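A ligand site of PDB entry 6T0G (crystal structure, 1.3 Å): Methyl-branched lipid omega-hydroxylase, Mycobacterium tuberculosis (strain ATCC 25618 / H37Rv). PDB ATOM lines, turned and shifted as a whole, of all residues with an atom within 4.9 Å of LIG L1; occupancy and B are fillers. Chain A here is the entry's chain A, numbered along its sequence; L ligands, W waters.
SG of Cys 386 binds FE1 of LIG L1, at 2.3 Å. NE2 of His 125 sits at hydrogen-bond distance from O4 of LIG L1 (2.5 Å). An oxygen (O3) of LIG L1 sits at hydrogen-bond distance from a ring nitrogen (ND1) of His 384 (2.7 Å). NH2 of Arg 327 lies within salt-bridge range of O1 of LIG L1 (2.8 Å). O4 of LIG L1 lies within salt-bridge range of NH1 of Arg 129 (2.8 Å).
Water W1 lies within hydrogen-bond range of an oxygen (O1) of LIG L1 (2.6 Å), the guanidinium group of Arg 327 (3.1 Å) and the side-chain sulfur of Met 325 (3.2 Å). Water W4 lies within hydrogen-bond range of an oxygen (O2) of LIG L1 (2.7 Å), the backbone carbonyl oxygen (O) of Phe 378 (2.9 Å), the backbone NH (N) of Gly 381 (3.0 Å) and the backbone NH (N) of Gly 380 (3.3 Å). Water W3 lies within hydrogen-bond range of an oxygen (O2) of LIG L1, the side-chain hydroxyl of Tyr 350 and the backbone NH of Gly 380. Water W2 lies within hydrogen-bond range of O2 of LIG L1, N of His 384 and O of Gly 381.
The side-chain sulfur (SG) of Cys 386 sits close to the backbone NH (N) of Gly 388, at 3.3 Å. N of Cys 386 lies within hydrogen-bond range of O of Phe 378. NE2 of His 125 lies within hydrogen-bond range of ND1 of His 384, at 3.3 Å. O of Phe 385 sits at hydrogen-bond distance from NH1 of Arg 129 (2.8 Å). The backbone NH (N) of Arg 129 sits close to the side-chain sulfur (SD) of Met 117. OG1 of Thr 278 is in hydrogen-bond range of O of Ala 274 (2.6 Å). OG1 of Thr 279 sits at hydrogen-bond distance from OE1 of Glu 395 (3.0 Å).
Residues that only touch LIG L1: Leu 271 (3.1 Å), Thr 278 (3.1 Å), Gly 377 (3.3 Å), Ala 274 (3.4 Å), Ile 118 (3.5 Å), Gly 388 (3.6 Å), Thr 279 (3.6 Å), Phe 378 (3.6 Å), Gly 379 (3.6 Å), Val 322 (3.6 Å), Tyr 350 (3.7 Å), Gly 275 (3.7 Å), Ile 183 (3.7 Å), Pro 321 (3.7 Å), Ala 392 (3.7 Å), Leu 387 (3.8 Å), Ala 383 (3.9 Å), Glu 395 (3.9 Å), Met 325 (3.9 Å), Leu 270 (3.97 Å), Phe 385 (3.997 Å) and Ala 282 (3.998 Å). Hydrophobic or aromatic side chains that line LIG L1: Ile 118, His 125, Ile 183, Leu 270, Ala 274, Ala 282, Pro 321, Val 322, Met 325, Tyr 350, Phe 378, His 384, Leu 387 and Ala 392. Of the 34 residues printed, 27 come within 4 Å of LIG L1. The nearest printed residue that does not touch LIG L1 is Met 117 (4.04 Å).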
ATOM      1  N   MET A 117       0.263 -10.868   8.228  1.00  0.00           N
ATOM      2  CA  MET A 117       0.739 -10.698   6.872  1.00  0.00           C
ATOM      3  C   MET A 117       1.486 -11.908   6.347  1.00  0.00           C
ATOM      4  O   MET A 117       1.672 -12.008   5.127  1.00  0.00           O
ATOM      5  CB  MET A 117       1.635  -9.451   6.776  1.00  0.00           C
ATOM      6  CG  MET A 117       2.952  -9.654   7.447  1.00  0.00           C
ATOM      7  SD  MET A 117       3.822  -8.051   7.454  1.00  0.00           S
ATOM      8  CE  MET A 117       5.361  -8.486   8.205  1.00  0.00           C
ATOM      9  N   ILE A 118       1.939 -12.823   7.212  1.00  0.00           N
ATOM     10  CA  ILE A 118       2.734 -13.933   6.720  1.00  0.00           C
ATOM     11  C   ILE A 118       1.819 -14.926   6.031  1.00  0.00           C
ATOM     12  O   ILE A 118       2.282 -15.781   5.284  1.00  0.00           O
ATOM     13  CB  ILE A 118       3.545 -14.577   7.874  1.00  0.00           C
ATOM     14  CG1 ILE A 118       4.743 -15.337   7.315  1.00  0.00           C
ATOM     15  CG2 ILE A 118       2.666 -15.490   8.735  1.00  0.00           C
ATOM     16  CD1 ILE A 118       5.717 -15.903   8.408  1.00  0.00           C
ATOM     17  N   HIS A 125      -0.455  -7.860   1.898  1.00  0.00           N
ATOM     18  CA  HIS A 125       0.775  -8.207   2.620  1.00  0.00           C
ATOM     19  C   HIS A 125       1.742  -7.028   2.642  1.00  0.00           C
ATOM     20  O   HIS A 125       2.270  -6.706   3.697  1.00  0.00           O
ATOM     21  CB  HIS A 125       1.435  -9.439   2.018  1.00  0.00           C
ATOM     22  CG  HIS A 125       2.893  -9.530   2.349  1.00  0.00           C
ATOM     23  ND1 HIS A 125       3.878  -9.049   1.524  1.00  0.00           N
ATOM     24  CD2 HIS A 125       3.536  -9.998   3.461  1.00  0.00           C
ATOM     25  CE1 HIS A 125       5.061  -9.227   2.086  1.00  0.00           C
ATOM     26  NE2 HIS A 125       4.885  -9.797   3.269  1.00  0.00           N
ATOM     27  N   ARG A 129       3.207  -4.909   5.804  1.00  0.00           N
ATOM     28  CA  ARG A 129       4.628  -4.934   6.084  1.00  0.00           C
ATOM     29  C   ARG A 129       5.206  -3.543   6.130  1.00  0.00           C
ATOM     30  O   ARG A 129       6.104  -3.263   6.949  1.00  0.00           O
ATOM     31  CB  ARG A 129       5.335  -5.766   5.028  1.00  0.00           C
ATOM     32  CG  ARG A 129       6.861  -5.898   5.281  1.00  0.00           C
ATOM     33  CD  ARG A 129       7.481  -7.056   4.501  1.00  0.00           C
ATOM     34  NE  ARG A 129       8.934  -7.021   4.506  1.00  0.00           N
ATOM     35  CZ  ARG A 129       9.719  -8.105   4.447  1.00  0.00           C
ATOM     36  NH1 ARG A 129       9.224  -9.313   4.463  1.00  0.00           N
ATOM     37  NH2 ARG A 129      11.017  -7.953   4.437  1.00  0.00           N
ATOM     38  N   PHE A 136      13.111  -2.234  10.673  1.00  0.00           N
ATOM     39  CA  PHE A 136      13.919  -3.429  10.463  1.00  0.00           C
ATOM     40  C   PHE A 136      14.988  -3.254   9.388  1.00  0.00           C
ATOM     41  O   PHE A 136      15.732  -4.200   9.106  1.00  0.00           O
ATOM     42  CB  PHE A 136      13.019  -4.632  10.126  1.00  0.00           C
ATOM     43  CG  PHE A 136      12.192  -5.087  11.304  1.00  0.00           C
ATOM     44  CD1 PHE A 136      12.694  -6.011  12.210  1.00  0.00           C
ATOM     45  CD2 PHE A 136      10.913  -4.554  11.541  1.00  0.00           C
ATOM     46  CE1 PHE A 136      11.947  -6.406  13.264  1.00  0.00           C
ATOM     47  CE2 PHE A 136      10.188  -4.954  12.597  1.00  0.00           C
ATOM     48  CZ  PHE A 136      10.700  -5.857  13.482  1.00  0.00           C
ATOM     49  N   ILE A 183      13.560  -7.748  20.706  1.00  0.00           N
ATOM     50  CA  ILE A 183      12.253  -7.593  20.069  1.00  0.00           C
ATOM     51  C   ILE A 183      11.232  -7.013  21.043  1.00  0.00           C
ATOM     52  O   ILE A 183      10.432  -6.171  20.647  1.00  0.00           O
ATOM     53  CB  ILE A 183      11.801  -8.887  19.356  1.00  0.00           C
ATOM     54  CG1 ILE A 183      10.579  -8.650  18.456  1.00  0.00           C
ATOM     55  CG2 ILE A 183      11.442 -10.000  20.356  1.00  0.00           C
ATOM     56  CD1 ILE A 183      10.793  -7.673  17.337  1.00  0.00           C
ATOM     57  N   LEU A 270       2.963 -12.214  15.598  1.00  0.00           N
ATOM     58  CA  LEU A 270       3.917 -12.611  14.585  1.00  0.00           C
ATOM     59  C   LEU A 270       5.293 -12.073  14.904  1.00  0.00           C
ATOM     60  O   LEU A 270       6.290 -12.785  14.774  1.00  0.00           O
ATOM     61  CB  LEU A 270       3.465 -12.069  13.228  1.00  0.00           C
ATOM     62  CG  LEU A 270       4.495 -12.139  12.088  1.00  0.00           C
ATOM     63  CD1 LEU A 270       4.959 -13.575  11.714  1.00  0.00           C
ATOM     64  CD2 LEU A 270       3.943 -11.416  10.871  1.00  0.00           C
ATOM     65  N   LEU A 271       5.386 -10.803  15.292  1.00  0.00           N
ATOM     66  CA  LEU A 271       6.692 -10.206  15.525  1.00  0.00           C
ATOM     67  C   LEU A 271       7.381 -10.810  16.734  1.00  0.00           C
ATOM     68  O   LEU A 271       8.589 -11.077  16.690  1.00  0.00           O
ATOM     69  CB  LEU A 271       6.554  -8.696  15.672  1.00  0.00           C
ATOM     70  CG  LEU A 271       6.143  -7.980  14.376  1.00  0.00           C
ATOM     71  CD1 LEU A 271       5.765  -6.481  14.652  1.00  0.00           C
ATOM     72  CD2 LEU A 271       7.224  -8.034  13.338  1.00  0.00           C
ATOM     73  N   ALA A 274       8.266 -14.681  15.913  1.00  0.00           N
ATOM     74  CA  ALA A 274       9.415 -14.775  15.019  1.00  0.00           C
ATOM     75  C   ALA A 274      10.681 -14.273  15.704  1.00  0.00           C
ATOM     76  O   ALA A 274      11.759 -14.830  15.515  1.00  0.00           O
ATOM     77  CB  ALA A 274       9.120 -13.970  13.775  1.00  0.00           C
ATOM     78  N   GLY A 275      10.575 -13.242  16.510  1.00  0.00           N
ATOM     79  CA  GLY A 275      11.746 -12.696  17.176  1.00  0.00           C
ATOM     80  C   GLY A 275      12.326 -13.594  18.242  1.00  0.00           C
ATOM     81  O   GLY A 275      13.522 -13.553  18.510  1.00  0.00           O
ATOM     82  N   THR A 278      13.645 -18.112  16.763  1.00  0.00           N
ATOM     83  CA  THR A 278      14.491 -18.296  15.554  1.00  0.00           C
ATOM     84  C   THR A 278      15.972 -18.041  15.888  1.00  0.00           C
ATOM     85  O   THR A 278      16.763 -18.980  15.865  1.00  0.00           O
ATOM     86  CB  THR A 278      14.028 -17.324  14.462  1.00  0.00           C
ATOM     87  OG1 THR A 278      14.053 -15.993  14.999  1.00  0.00           O
ATOM     88  CG2 THR A 278      12.644 -17.617  13.917  1.00  0.00           C
ATOM     89  N   THR A 279      16.321 -16.802  16.185  1.00  0.00           N
ATOM     90  CA  THR A 279      17.720 -16.484  16.420  1.00  0.00           C
ATOM     91  C   THR A 279      18.303 -17.303  17.554  1.00  0.00           C
ATOM     92  O   THR A 279      19.462 -17.729  17.480  1.00  0.00           O
ATOM     93  CB  THR A 279      17.842 -15.014  16.764  1.00  0.00           C
ATOM     94  OG1 THR A 279      17.162 -14.265  15.768  1.00  0.00           O
ATOM     95  CG2 THR A 279      19.323 -14.603  16.824  1.00  0.00           C
ATOM     96  N   ALA A 282      19.664 -20.334  16.002  1.00  0.00           N
ATOM     97  CA  ALA A 282      20.889 -20.068  15.294  1.00  0.00           C
ATOM     98  C   ALA A 282      22.061 -19.995  16.265  1.00  0.00           C
ATOM     99  O   ALA A 282      23.140 -20.553  16.017  1.00  0.00           O
ATOM    100  CB  ALA A 282      20.806 -18.790  14.480  1.00  0.00           C
ATOM    101  N   VAL A 316      23.642 -19.732   9.949  1.00  0.00           N
ATOM    102  CA  VAL A 316      22.252 -19.801   9.565  1.00  0.00           C
ATOM    103  C   VAL A 316      22.031 -20.953   8.573  1.00  0.00           C
ATOM    104  O   VAL A 316      21.072 -21.723   8.726  1.00  0.00           O
ATOM    105  CB  VAL A 316      21.711 -18.449   9.057  1.00  0.00           C
ATOM    106  CG1 VAL A 316      20.273 -18.610   8.610  1.00  0.00           C
ATOM    107  CG2 VAL A 316      21.794 -17.393  10.187  1.00  0.00           C
ATOM    108  N   PRO A 321      17.266 -22.623  11.047  1.00  0.00           N
ATOM    109  CA  PRO A 321      16.353 -22.547  12.215  1.00  0.00           C
ATOM    110  C   PRO A 321      14.900 -22.724  11.884  1.00  0.00           C
ATOM    111  O   PRO A 321      14.154 -23.264  12.716  1.00  0.00           O
ATOM    112  CB  PRO A 321      16.627 -21.160  12.790  1.00  0.00           C
ATOM    113  CG  PRO A 321      18.066 -20.939  12.394  1.00  0.00           C
ATOM    114  CD  PRO A 321      18.163 -21.471  10.980  1.00  0.00           C
ATOM    115  N   VAL A 322      14.488 -22.309  10.698  1.00  0.00           N
ATOM    116  CA  VAL A 322      13.144 -22.549  10.180  1.00  0.00           C
ATOM    117  C   VAL A 322      13.270 -23.678   9.147  1.00  0.00           C
ATOM    118  O   VAL A 322      13.942 -23.555   8.145  1.00  0.00           O
ATOM    119  CB  VAL A 322      12.534 -21.278   9.576  1.00  0.00           C
ATOM    120  CG1 VAL A 322      11.174 -21.577   8.974  1.00  0.00           C
ATOM    121  CG2 VAL A 322      12.379 -20.181  10.643  1.00  0.00           C
ATOM    122  N   MET A 325       8.705 -23.847   5.008  1.00  0.00           N
ATOM    123  CA  MET A 325       7.472 -23.072   4.984  1.00  0.00           C
ATOM    124  C   MET A 325       6.554 -23.688   3.923  1.00  0.00           C
ATOM    125  O   MET A 325       7.031 -24.285   2.951  1.00  0.00           O
ATOM    126  CB  MET A 325       7.686 -21.580   4.681  1.00  0.00           C
ATOM    127  CG  MET A 325       8.254 -20.769   5.847  1.00  0.00           C
ATOM    128  SD  MET A 325       6.984 -20.169   6.920  1.00  0.00           S
ATOM    129  CE  MET A 325       8.008 -19.386   8.179  1.00  0.00           C
ATOM    130  N   ARG A 327       3.258 -23.390   1.093  1.00  0.00           N
ATOM    131  CA  ARG A 327       2.522 -22.560   0.166  1.00  0.00           C
ATOM    132  C   ARG A 327       1.355 -23.376  -0.337  1.00  0.00           C
ATOM    133  O   ARG A 327       1.283 -24.585  -0.090  1.00  0.00           O
ATOM    134  CB  ARG A 327       3.396 -22.143  -1.012  1.00  0.00           C
ATOM    135  CG  ARG A 327       4.636 -21.336  -0.616  1.00  0.00           C
ATOM    136  CD  ARG A 327       4.263 -19.953  -0.206  1.00  0.00           C
ATOM    137  NE  ARG A 327       5.385 -19.031  -0.039  1.00  0.00           N
ATOM    138  CZ  ARG A 327       5.954 -18.728   1.119  1.00  0.00           C
ATOM    139  NH1 ARG A 327       5.632 -19.410   2.231  1.00  0.00           N
ATOM    140  NH2 ARG A 327       6.878 -17.765   1.161  1.00  0.00           N
ATOM    141  N   TYR A 350      13.747 -25.773   3.504  1.00  0.00           N
ATOM    142  CA  TYR A 350      14.990 -25.013   3.582  1.00  0.00           C
ATOM    143  C   TYR A 350      16.131 -25.854   4.134  1.00  0.00           C
ATOM    144  O   TYR A 350      17.276 -25.693   3.735  1.00  0.00           O
ATOM    145  CB  TYR A 350      14.808 -23.763   4.450  1.00  0.00           C
ATOM    146  CG  TYR A 350      13.621 -22.872   4.079  1.00  0.00           C
ATOM    147  CD1 TYR A 350      13.489 -22.326   2.817  1.00  0.00           C
ATOM    148  CD2 TYR A 350      12.643 -22.535   5.042  1.00  0.00           C
ATOM    149  CE1 TYR A 350      12.423 -21.551   2.477  1.00  0.00           C
ATOM    150  CE2 TYR A 350      11.558 -21.762   4.744  1.00  0.00           C
ATOM    151  CZ  TYR A 350      11.473 -21.215   3.469  1.00  0.00           C
ATOM    152  OH  TYR A 350      10.424 -20.406   3.164  1.00  0.00           O
ATOM    153  N   GLY A 377      18.219 -20.040   4.437  1.00  0.00           N
ATOM    154  CA  GLY A 377      17.799 -20.008   5.838  1.00  0.00           C
ATOM    155  C   GLY A 377      16.789 -18.931   6.184  1.00  0.00           C
ATOM    156  O   GLY A 377      15.955 -19.131   7.084  1.00  0.00           O
ATOM    157  N   PHE A 378      16.853 -17.774   5.497  1.00  0.00           N
ATOM    158  CA  PHE A 378      15.880 -16.699   5.627  1.00  0.00           C
ATOM    159  C   PHE A 378      14.807 -16.775   4.536  1.00  0.00           C
ATOM    160  O   PHE A 378      14.063 -15.808   4.350  1.00  0.00           O
ATOM    161  CB  PHE A 378      16.622 -15.361   5.551  1.00  0.00           C
ATOM    162  CG  PHE A 378      17.531 -15.086   6.685  1.00  0.00           C
ATOM    163  CD1 PHE A 378      17.038 -14.973   7.975  1.00  0.00           C
ATOM    164  CD2 PHE A 378      18.913 -14.920   6.467  1.00  0.00           C
ATOM    165  CE1 PHE A 378      17.897 -14.678   9.016  1.00  0.00           C
ATOM    166  CE2 PHE A 378      19.779 -14.636   7.516  1.00  0.00           C
ATOM    167  CZ  PHE A 378      19.249 -14.504   8.798  1.00  0.00           C
ATOM    168  N   GLY A 379      14.706 -17.913   3.858  1.00  0.00           N
ATOM    169  CA  GLY A 379      13.816 -18.127   2.739  1.00  0.00           C
ATOM    170  C   GLY A 379      14.533 -17.981   1.398  1.00  0.00           C
ATOM    171  O   GLY A 379      15.716 -17.654   1.311  1.00  0.00           O
ATOM    172  N   GLY A 380      13.761 -18.160   0.347  1.00  0.00           N
ATOM    173  CA  GLY A 380      14.214 -18.093  -1.026  1.00  0.00           C
ATOM    174  C   GLY A 380      14.296 -16.712  -1.617  1.00  0.00           C
ATOM    175  O   GLY A 380      14.741 -16.533  -2.753  1.00  0.00           O
ATOM    176  N   GLY A 381      13.919 -15.711  -0.863  1.00  0.00           N
ATOM    177  CA  GLY A 381      13.842 -14.353  -1.373  1.00  0.00           C
ATOM    178  C   GLY A 381      12.445 -14.033  -1.819  1.00  0.00           C
ATOM    179  O   GLY A 381      11.531 -14.866  -1.809  1.00  0.00           O
ATOM    180  N   ALA A 383       8.795 -11.802  -1.796  1.00  0.00           N
ATOM    181  CA  ALA A 383       7.869 -10.923  -1.088  1.00  0.00           C
ATOM    182  C   ALA A 383       7.933 -11.102   0.426  1.00  0.00           C
ATOM    183  O   ALA A 383       7.777 -10.116   1.185  1.00  0.00           O
ATOM    184  CB  ALA A 383       6.448 -11.148  -1.626  1.00  0.00           C
ATOM    185  N   HIS A 384       8.151 -12.315   0.908  1.00  0.00           N
ATOM    186  CA  HIS A 384       8.118 -12.585   2.350  1.00  0.00           C
ATOM    187  C   HIS A 384       9.505 -12.736   2.936  1.00  0.00           C
ATOM    188  O   HIS A 384       9.621 -13.186   4.086  1.00  0.00           O
ATOM    189  CB  HIS A 384       7.236 -13.795   2.680  1.00  0.00           C
ATOM    190  CG  HIS A 384       5.795 -13.590   2.357  1.00  0.00           C
ATOM    191  ND1 HIS A 384       4.845 -13.146   3.281  1.00  0.00           N
ATOM    192  CD2 HIS A 384       5.125 -13.833   1.223  1.00  0.00           C
ATOM    193  CE1 HIS A 384       3.666 -13.119   2.681  1.00  0.00           C
ATOM    194  NE2 HIS A 384       3.807 -13.538   1.445  1.00  0.00           N
ATOM    195  N   PHE A 385      10.553 -12.370   2.223  1.00  0.00           N
ATOM    196  CA  PHE A 385      11.886 -12.536   2.766  1.00  0.00           C
ATOM    197  C   PHE A 385      11.968 -12.012   4.203  1.00  0.00           C
ATOM    198  O   PHE A 385      11.515 -10.909   4.519  1.00  0.00           O
ATOM    199  CB  PHE A 385      12.907 -11.825   1.891  1.00  0.00           C
ATOM    200  CG  PHE A 385      14.311 -12.034   2.378  1.00  0.00           C
ATOM    201  CD1 PHE A 385      15.012 -13.188   2.086  1.00  0.00           C
ATOM    202  CD2 PHE A 385      14.896 -11.108   3.250  1.00  0.00           C
ATOM    203  CE1 PHE A 385      16.281 -13.372   2.605  1.00  0.00           C
ATOM    204  CE2 PHE A 385      16.129 -11.343   3.756  1.00  0.00           C
ATOM    205  CZ  PHE A 385      16.800 -12.479   3.432  1.00  0.00           C
ATOM    206  N   CYS A 386      12.572 -12.807   5.063  1.00  0.00           N
ATOM    207  CA  CYS A 386      12.600 -12.544   6.492  1.00  0.00           C
ATOM    208  C   CYS A 386      12.758 -11.069   6.811  1.00  0.00           C
ATOM    209  O   CYS A 386      13.821 -10.480   6.555  1.00  0.00           O
ATOM    210  CB  CYS A 386      13.753 -13.329   7.114  1.00  0.00           C
ATOM    211  SG  CYS A 386      13.916 -12.930   8.894  1.00  0.00           S
ATOM    212  N   LEU A 387      11.732 -10.509   7.458  1.00  0.00           N
ATOM    213  CA  LEU A 387      11.740  -9.118   7.872  1.00  0.00           C
ATOM    214  C   LEU A 387      12.856  -8.865   8.875  1.00  0.00           C
ATOM    215  O   LEU A 387      13.394  -7.756   8.929  1.00  0.00           O
ATOM    216  CB  LEU A 387      10.389  -8.769   8.494  1.00  0.00           C
ATOM    217  CG  LEU A 387      10.272  -7.334   9.000  1.00  0.00           C
ATOM    218  CD1 LEU A 387      10.350  -6.324   7.881  1.00  0.00           C
ATOM    219  CD2 LEU A 387       8.947  -7.212   9.825  1.00  0.00           C
ATOM    220  N   GLY A 388      13.128  -9.829   9.721  1.00  0.00           N
ATOM    221  CA  GLY A 388      14.095  -9.723  10.783  1.00  0.00           C
ATOM    222  C   GLY A 388      15.514 -10.123  10.418  1.00  0.00           C
ATOM    223  O   GLY A 388      16.353 -10.209  11.320  1.00  0.00           O
ATOM    224  N   LEU A 391      18.253  -7.764  11.780  1.00  0.00           N
ATOM    225  CA  LEU A 391      18.205  -7.895  13.227  1.00  0.00           C
ATOM    226  C   LEU A 391      18.842  -9.200  13.688  1.00  0.00           C
ATOM    227  O   LEU A 391      19.684  -9.192  14.599  1.00  0.00           O
ATOM    228  CB  LEU A 391      16.757  -7.750  13.711  1.00  0.00           C
ATOM    229  CG  LEU A 391      16.614  -7.859  15.232  1.00  0.00           C
ATOM    230  CD1 LEU A 391      17.389  -6.790  15.945  1.00  0.00           C
ATOM    231  CD2 LEU A 391      15.140  -7.849  15.587  1.00  0.00           C
ATOM    232  N   ALA A 392      18.466 -10.331  13.073  1.00  0.00           N
ATOM    233  CA  ALA A 392      18.981 -11.641  13.471  1.00  0.00           C
ATOM    234  C   ALA A 392      20.493 -11.722  13.270  1.00  0.00           C
ATOM    235  O   ALA A 392      21.215 -12.229  14.132  1.00  0.00           O
ATOM    236  CB  ALA A 392      18.314 -12.736  12.637  1.00  0.00           C
ATOM    237  N   GLU A 395      22.135  -9.796  16.069  1.00  0.00           N
ATOM    238  CA  GLU A 395      22.014 -10.507  17.347  1.00  0.00           C
ATOM    239  C   GLU A 395      23.028 -11.641  17.414  1.00  0.00           C
ATOM    240  O   GLU A 395      23.641 -11.899  18.452  1.00  0.00           O
ATOM    241  CB  GLU A 395      20.587 -11.069  17.494  1.00  0.00           C
ATOM    242  CG  GLU A 395      19.482 -10.032  17.716  1.00  0.00           C
ATOM    243  CD  GLU A 395      18.075 -10.607  17.660  1.00  0.00           C
ATOM    244  OE1 GLU A 395      17.823 -11.627  16.982  1.00  0.00           O
ATOM    245  OE2 GLU A 395      17.169  -9.913  18.198  1.00  0.00           O
ATOM    246  N   ILE A 396      23.147 -12.404  16.330  1.00  0.00           N
ATOM    247  CA  ILE A 396      24.095 -13.517  16.277  1.00  0.00           C
ATOM    248  C   ILE A 396      25.517 -13.012  16.413  1.00  0.00           C
ATOM    249  O   ILE A 396      26.308 -13.514  17.234  1.00  0.00           O
ATOM    250  CB  ILE A 396      23.888 -14.334  14.975  1.00  0.00           C
ATOM    251  CG1 ILE A 396      22.516 -14.988  14.930  1.00  0.00           C
ATOM    252  CG2 ILE A 396      24.998 -15.374  14.871  1.00  0.00           C
ATOM    253  CD1 ILE A 396      22.117 -15.430  13.519  1.00  0.00           C
HETATM  254  C1  LIG L   1       9.816 -14.595   7.796  1.00  0.00           C
HETATM  255  C2  LIG L   1      13.729 -17.245   8.960  1.00  0.00           C
HETATM  256  C3  LIG L   1      14.741 -14.115  12.586  1.00  0.00           C
HETATM  257  C4  LIG L   1      10.612 -11.731  11.634  1.00  0.00           C
HETATM  258  C5  LIG L   1      10.824 -15.589   7.777  1.00  0.00           C
HETATM  259  C6  LIG L   1      10.863 -16.718   6.877  1.00  0.00           C
HETATM  260  C7  LIG L   1      11.958 -17.453   7.234  1.00  0.00           C
HETATM  261  C8  LIG L   1      12.578 -16.800   8.321  1.00  0.00           C
HETATM  262  C9  LIG L   1      12.478 -18.722   6.592  1.00  0.00           C
HETATM  263  C10 LIG L   1       9.915 -16.992   5.724  1.00  0.00           C
HETATM  264  C11 LIG L   1      10.500 -16.314   4.456  1.00  0.00           C
HETATM  265  C12 LIG L   1       9.664 -16.598   3.216  1.00  0.00           C
HETATM  266  O1  LIG L   1       8.472 -17.034   3.321  1.00  0.00           O
HETATM  267  O2  LIG L   1      10.159 -16.345   2.086  1.00  0.00           O
HETATM  268  C13 LIG L   1      14.333 -16.620  10.063  1.00  0.00           C
HETATM  269  C14 LIG L   1      15.530 -17.099  10.680  1.00  0.00           C
HETATM  270  C15 LIG L   1      15.866 -16.239  11.707  1.00  0.00           C
HETATM  271  C16 LIG L   1      14.822 -15.196  11.676  1.00  0.00           C
HETATM  272  C17 LIG L   1      16.293 -18.326  10.242  1.00  0.00           C
HETATM  273  C18 LIG L   1      17.009 -16.242  12.652  1.00  0.00           C
HETATM  274  C19 LIG L   1      18.258 -16.610  12.303  1.00  0.00           C
HETATM  275  C20 LIG L   1      13.685 -13.216  12.704  1.00  0.00           C
HETATM  276  C21 LIG L   1      13.618 -12.158  13.651  1.00  0.00           C
HETATM  277  C22 LIG L   1      12.417 -11.516  13.394  1.00  0.00           C
HETATM  278  C23 LIG L   1      11.812 -12.152  12.249  1.00  0.00           C
HETATM  279  C24 LIG L   1      14.653 -11.890  14.761  1.00  0.00           C
HETATM  280  C25 LIG L   1      11.914 -10.352  14.202  1.00  0.00           C
HETATM  281  C26 LIG L   1      10.636 -10.116  14.541  1.00  0.00           C
HETATM  282  C27 LIG L   1      10.073 -12.304  10.492  1.00  0.00           C
HETATM  283  C28 LIG L   1       8.781 -11.867   9.913  1.00  0.00           C
HETATM  284  C29 LIG L   1       8.523 -12.674   8.851  1.00  0.00           C
HETATM  285  C30 LIG L   1       9.701 -13.600   8.779  1.00  0.00           C
HETATM  286  C31 LIG L   1       7.863 -10.792  10.464  1.00  0.00           C
HETATM  287  C32 LIG L   1       7.327 -12.587   7.907  1.00  0.00           C
HETATM  288  C33 LIG L   1       7.719 -11.640   6.739  1.00  0.00           C
HETATM  289  C34 LIG L   1       6.619 -11.428   5.723  1.00  0.00           C
HETATM  290  O3  LIG L   1       5.661 -12.235   5.726  1.00  0.00           O
HETATM  291  O4  LIG L   1       6.704 -10.493   4.879  1.00  0.00           O
HETATM  292  N1  LIG L   1      11.872 -15.686   8.672  1.00  0.00           N
HETATM  293  N2  LIG L   1      13.888 -15.510  10.701  1.00  0.00           N
HETATM  294  N3  LIG L   1      12.615 -13.183  11.861  1.00  0.00           N
HETATM  295  N4  LIG L   1      10.602 -13.372   9.826  1.00  0.00           N
HETATM  296 FE1  LIG L   1      12.388 -14.263  10.079  1.00  0.00          FE
HETATM  297  C1  LG2 L   2      -1.273 -23.038  12.126  1.00  0.00           C
HETATM  298  C2  LG2 L   2      -0.514 -21.789  12.073  1.00  0.00           C
HETATM  299  C3  LG2 L   2       0.151 -21.277  13.125  1.00  0.00           C
HETATM  300  C4  LG2 L   2       0.192 -21.886  14.531  1.00  0.00           C
HETATM  301  C5  LG2 L   2       1.540 -21.631  15.245  1.00  0.00           C
HETATM  302  C6  LG2 L   2       2.105 -20.217  15.033  1.00  0.00           C
HETATM  303  C7  LG2 L   2       2.209 -19.937  13.542  1.00  0.00           C
HETATM  304  C8  LG2 L   2       0.819 -19.966  12.924  1.00  0.00           C
HETATM  305  C9  LG2 L   2       0.883 -19.399  11.505  1.00  0.00           C
HETATM  306  C10 LG2 L   2       1.914 -18.279  11.717  1.00  0.00           C
HETATM  307  C11 LG2 L   2       2.402 -18.457  13.159  1.00  0.00           C
HETATM  308  C12 LG2 L   2       3.224 -20.849  12.847  1.00  0.00           C
HETATM  309  C13 LG2 L   2       3.790 -17.846  13.546  1.00  0.00           C
HETATM  310  C14 LG2 L   2       3.631 -16.415  14.041  1.00  0.00           C
HETATM  311  C15 LG2 L   2       4.750 -17.667  12.380  1.00  0.00           C
HETATM  312  C16 LG2 L   2       6.218 -17.647  12.847  1.00  0.00           C
HETATM  313  C17 LG2 L   2       7.199 -17.410  11.719  1.00  0.00           C
HETATM  314  C18 LG2 L   2       8.640 -17.460  12.152  1.00  0.00           C
HETATM  315  C19 LG2 L   2       9.058 -18.883  12.488  1.00  0.00           C
HETATM  316  C20 LG2 L   2       9.589 -16.965  11.047  1.00  0.00           C
HETATM  317  O   HOH W   1       6.417 -17.867   4.746  1.00  0.00           O
HETATM  318  O   HOH W   2       9.186 -14.872  -0.025  1.00  0.00           O
HETATM  319  O   HOH W   3      10.930 -18.711   1.053  1.00  0.00           O
HETATM  320  O   HOH W   4      12.674 -15.444   1.815  1.00  0.00           O
